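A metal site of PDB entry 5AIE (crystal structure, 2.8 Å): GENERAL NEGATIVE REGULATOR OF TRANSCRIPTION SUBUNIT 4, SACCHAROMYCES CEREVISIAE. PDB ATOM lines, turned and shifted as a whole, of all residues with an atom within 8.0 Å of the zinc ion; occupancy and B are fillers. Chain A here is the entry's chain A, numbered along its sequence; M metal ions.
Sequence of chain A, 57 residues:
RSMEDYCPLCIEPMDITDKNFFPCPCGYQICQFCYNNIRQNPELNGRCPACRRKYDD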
ATOM      1  N   PRO A  23      12.193  30.185 -16.417  1.00  0.00           N
ATOM      2  CA  PRO A  23      11.731  28.888 -16.906  1.00  0.00           C
ATOM      3  C   PRO A  23      10.903  28.974 -18.189  1.00  0.00           C
ATOM      4  O   PRO A  23      10.808  27.988 -18.927  1.00  0.00           O
ATOM      5  CB  PRO A  23      10.882  28.359 -15.741  1.00  0.00           C
ATOM      6  CG  PRO A  23      10.434  29.581 -15.033  1.00  0.00           C
ATOM      7  CD  PRO A  23      11.564  30.557 -15.145  1.00  0.00           C
ATOM      8  N   CYS A  24      10.317  30.136 -18.449  1.00  0.00           N
ATOM      9  CA  CYS A  24       9.501  30.338 -19.638  1.00  0.00           C
ATOM     10  C   CYS A  24       9.926  31.606 -20.366  1.00  0.00           C
ATOM     11  O   CYS A  24      10.221  32.626 -19.732  1.00  0.00           O
ATOM     12  CB  CYS A  24       8.021  30.415 -19.244  1.00  0.00           C
ATOM     13  SG  CYS A  24       6.865  30.344 -20.629  1.00  0.00           S
ATOM     14  N   PRO A  25       9.974  31.557 -21.711  1.00  0.00           N
ATOM     15  CA  PRO A  25      10.361  32.696 -22.552  1.00  0.00           C
ATOM     16  C   PRO A  25       9.492  33.937 -22.366  1.00  0.00           C
ATOM     17  O   PRO A  25       9.882  35.028 -22.788  1.00  0.00           O
ATOM     18  CB  PRO A  25      10.229  32.149 -23.979  1.00  0.00           C
ATOM     19  CG  PRO A  25       9.414  30.895 -23.857  1.00  0.00           C
ATOM     20  CD  PRO A  25       9.763  30.337 -22.516  1.00  0.00           C
ATOM     21  N   CYS A  26       8.315  33.774 -21.756  1.00  0.00           N
ATOM     22  CA  CYS A  26       7.401  34.892 -21.561  1.00  0.00           C
ATOM     23  C   CYS A  26       7.910  35.858 -20.487  1.00  0.00           C
ATOM     24  O   CYS A  26       7.581  37.048 -20.505  1.00  0.00           O
ATOM     25  CB  CYS A  26       6.004  34.385 -21.188  1.00  0.00           C
ATOM     26  SG  CYS A  26       5.895  33.640 -19.557  1.00  0.00           S
ATOM     27  N   GLY A  27       8.698  35.336 -19.552  1.00  0.00           N
ATOM     28  CA  GLY A  27       9.287  36.166 -18.512  1.00  0.00           C
ATOM     29  C   GLY A  27       8.641  36.024 -17.148  1.00  0.00           C
ATOM     30  O   GLY A  27       9.062  36.668 -16.193  1.00  0.00           O
ATOM     31  N   TYR A  28       7.619  35.172 -17.058  1.00  0.00           N
ATOM     32  CA  TYR A  28       6.934  34.937 -15.797  1.00  0.00           C
ATOM     33  C   TYR A  28       7.837  34.164 -14.837  1.00  0.00           C
ATOM     34  O   TYR A  28       8.262  33.052 -15.140  1.00  0.00           O
ATOM     35  CB  TYR A  28       5.621  34.193 -16.033  1.00  0.00           C
ATOM     36  CG  TYR A  28       4.668  34.229 -14.860  1.00  0.00           C
ATOM     37  CD1 TYR A  28       4.043  35.411 -14.492  1.00  0.00           C
ATOM     38  CD2 TYR A  28       4.385  33.076 -14.132  1.00  0.00           C
ATOM     39  CE1 TYR A  28       3.171  35.450 -13.418  1.00  0.00           C
ATOM     40  CE2 TYR A  28       3.514  33.114 -13.058  1.00  0.00           C
ATOM     41  CZ  TYR A  28       2.911  34.301 -12.712  1.00  0.00           C
ATOM     42  OH  TYR A  28       2.037  34.347 -11.644  1.00  0.00           O
ATOM     43  N   GLN A  29       8.117  34.757 -13.680  1.00  0.00           N
ATOM     44  CA  GLN A  29       9.057  34.157 -12.732  1.00  0.00           C
ATOM     45  C   GLN A  29       8.372  33.573 -11.501  1.00  0.00           C
ATOM     46  O   GLN A  29       7.558  34.222 -10.856  1.00  0.00           O
ATOM     47  CB  GLN A  29      10.092  35.199 -12.297  1.00  0.00           C
ATOM     48  CG  GLN A  29      11.049  35.635 -13.381  1.00  0.00           C
ATOM     49  CD  GLN A  29      12.151  36.538 -12.865  1.00  0.00           C
ATOM     50  OE1 GLN A  29      11.899  37.691 -12.517  1.00  0.00           O
ATOM     51  NE2 GLN A  29      13.374  36.026 -12.805  1.00  0.00           N
ATOM     52  N   ARG A  47       2.799  23.499 -16.793  1.00  0.00           N
ATOM     53  CA  ARG A  47       3.054  24.568 -17.762  1.00  0.00           C
ATOM     54  C   ARG A  47       3.013  25.941 -17.091  1.00  0.00           C
ATOM     55  O   ARG A  47       2.571  26.056 -15.945  1.00  0.00           O
ATOM     56  CB  ARG A  47       2.051  24.498 -18.916  1.00  0.00           C
ATOM     57  CG  ARG A  47       0.626  24.181 -18.490  1.00  0.00           C
ATOM     58  CD  ARG A  47      -0.310  24.103 -19.686  1.00  0.00           C
ATOM     59  NE  ARG A  47       0.207  23.224 -20.735  1.00  0.00           N
ATOM     60  CZ  ARG A  47      -0.473  22.884 -21.826  1.00  0.00           C
ATOM     61  NH1 ARG A  47      -1.696  23.342 -22.011  1.00  0.00           N
ATOM     62  NH2 ARG A  47       0.082  22.079 -22.731  1.00  0.00           N
ATOM     63  N   CYS A  48       3.467  26.958 -17.801  1.00  0.00           N
ATOM     64  CA  CYS A  48       3.551  28.308 -17.247  1.00  0.00           C
ATOM     65  C   CYS A  48       2.172  28.879 -16.898  1.00  0.00           C
ATOM     66  O   CYS A  48       1.257  28.870 -17.725  1.00  0.00           O
ATOM     67  CB  CYS A  48       4.259  29.240 -18.237  1.00  0.00           C
ATOM     68  SG  CYS A  48       4.380  30.949 -17.675  1.00  0.00           S
ATOM     69  N   PRO A  49       2.030  29.381 -15.662  1.00  0.00           N
ATOM     70  CA  PRO A  49       0.774  29.959 -15.171  1.00  0.00           C
ATOM     71  C   PRO A  49       0.332  31.201 -15.946  1.00  0.00           C
ATOM     72  O   PRO A  49      -0.791  31.657 -15.754  1.00  0.00           O
ATOM     73  CB  PRO A  49       1.115  30.338 -13.717  1.00  0.00           C
ATOM     74  CG  PRO A  49       2.253  29.455 -13.356  1.00  0.00           C
ATOM     75  CD  PRO A  49       3.058  29.309 -14.615  1.00  0.00           C
ATOM     76  N   ALA A  50       1.191  31.727 -16.804  1.00  0.00           N
ATOM     77  CA  ALA A  50       0.868  32.914 -17.586  1.00  0.00           C
ATOM     78  C   ALA A  50       0.374  32.559 -18.988  1.00  0.00           C
ATOM     79  O   ALA A  50      -0.809  32.667 -19.271  1.00  0.00           O
ATOM     80  CB  ALA A  50       2.071  33.828 -17.660  1.00  0.00           C
ATOM     81  N   CYS A  51       1.293  32.140 -19.851  1.00  0.00           N
ATOM     82  CA  CYS A  51       0.967  31.911 -21.253  1.00  0.00           C
ATOM     83  C   CYS A  51       0.727  30.436 -21.574  1.00  0.00           C
ATOM     84  O   CYS A  51       0.620  30.060 -22.740  1.00  0.00           O
ATOM     85  CB  CYS A  51       2.076  32.453 -22.146  1.00  0.00           C
ATOM     86  SG  CYS A  51       3.655  31.584 -22.010  1.00  0.00           S
ATOM     87  N   ARG A  52       0.649  29.602 -20.533  1.00  0.00           N
ATOM     88  CA  ARG A  52       0.338  28.176 -20.670  1.00  0.00           C
ATOM     89  C   ARG A  52       1.315  27.416 -21.566  1.00  0.00           C
ATOM     90  O   ARG A  52       0.985  26.361 -22.097  1.00  0.00           O
ATOM     91  CB  ARG A  52      -1.082  27.998 -21.211  1.00  0.00           C
ATOM     92  CG  ARG A  52      -2.161  28.611 -20.339  1.00  0.00           C
ATOM     93  CD  ARG A  52      -3.550  28.261 -20.853  1.00  0.00           C
ATOM     94  NE  ARG A  52      -3.806  26.831 -20.783  1.00  0.00           N
ATOM     95  CZ  ARG A  52      -4.318  26.209 -19.724  1.00  0.00           C
ATOM     96  NH1 ARG A  52      -4.636  26.906 -18.642  1.00  0.00           N
ATOM     97  NH2 ARG A  52      -4.519  24.905 -19.743  1.00  0.00           N
ATOM     98  N   ARG A  53       2.531  27.955 -21.721  1.00  0.00           N
ATOM     99  CA  ARG A  53       3.536  27.296 -22.532  1.00  0.00           C
ATOM    100  C   ARG A  53       4.184  26.163 -21.730  1.00  0.00           C
ATOM    101  O   ARG A  53       4.534  26.331 -20.567  1.00  0.00           O
ATOM    102  CB  ARG A  53       4.608  28.299 -22.997  1.00  0.00           C
ATOM    103  CG  ARG A  53       5.321  27.898 -24.280  1.00  0.00           C
ATOM    104  CD  ARG A  53       6.396  28.919 -24.646  1.00  0.00           C
ATOM    105  NE  ARG A  53       5.834  30.224 -24.992  1.00  0.00           N
ATOM    106  CZ  ARG A  53       5.907  30.782 -26.200  1.00  0.00           C
ATOM    107  NH1 ARG A  53       6.511  30.132 -27.189  1.00  0.00           N
ATOM    108  NH2 ARG A  53       5.375  31.976 -26.417  1.00  0.00           N
ATOM    109  N   LYS A  54       4.320  25.003 -22.364  1.00  0.00           N
ATOM    110  CA  LYS A  54       4.861  23.826 -21.689  1.00  0.00           C
ATOM    111  C   LYS A  54       6.355  23.987 -21.392  1.00  0.00           C
ATOM    112  O   LYS A  54       7.118  24.494 -22.208  1.00  0.00           O
ATOM    113  CB  LYS A  54       4.639  22.570 -22.546  1.00  0.00           C
ATOM    114  N   TYR A  55       6.754  23.540 -20.203  1.00  0.00           N
ATOM    115  CA  TYR A  55       8.154  23.622 -19.793  1.00  0.00           C
ATOM    116  C   TYR A  55       9.005  22.575 -20.510  1.00  0.00           C
ATOM    117  O   TYR A  55       8.499  21.560 -20.991  1.00  0.00           O
ATOM    118  CB  TYR A  55       8.287  23.447 -18.281  1.00  0.00           C
ATOM    119  CG  TYR A  55       7.757  24.616 -17.483  1.00  0.00           C
ATOM    120  CD1 TYR A  55       8.401  25.841 -17.495  1.00  0.00           C
ATOM    121  CD2 TYR A  55       6.604  24.485 -16.705  1.00  0.00           C
ATOM    122  CE1 TYR A  55       7.916  26.903 -16.759  1.00  0.00           C
ATOM    123  CE2 TYR A  55       6.118  25.547 -15.969  1.00  0.00           C
ATOM    124  CZ  TYR A  55       6.786  26.755 -15.995  1.00  0.00           C
ATOM    125  OH  TYR A  55       6.306  27.824 -15.271  1.00  0.00           O
HETATM  126 ZN    ZN M   1       4.873  31.559 -20.020  1.00  0.00          ZN
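N of Cys 48 lies within hydrogen-bond range of O of Arg 53.
SG of Cys 48 lies close to N of Ala 50, at 3.4 Å.
The side-chain sulfur (SG) of Cys 26 lies close to the backbone NH (N) of Tyr 28 (3.4 Å).
Four residues have an atom within 4 Å of the zinc ion: Cys 24, Cys 26, Cys 48 and Cys 51.
Along chain A the residues within 4 Å of the zinc ion span positions 24 to 51.
The zinc ion is bound by the side-chain sulfur of Cys 51 (2.3 Å), the side-chain sulfur of Cys 26 (2.4 Å), the side-chain sulfur of Cys 24 (2.4 Å) and the side-chain sulfur of Cys 48 (2.5 Å).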
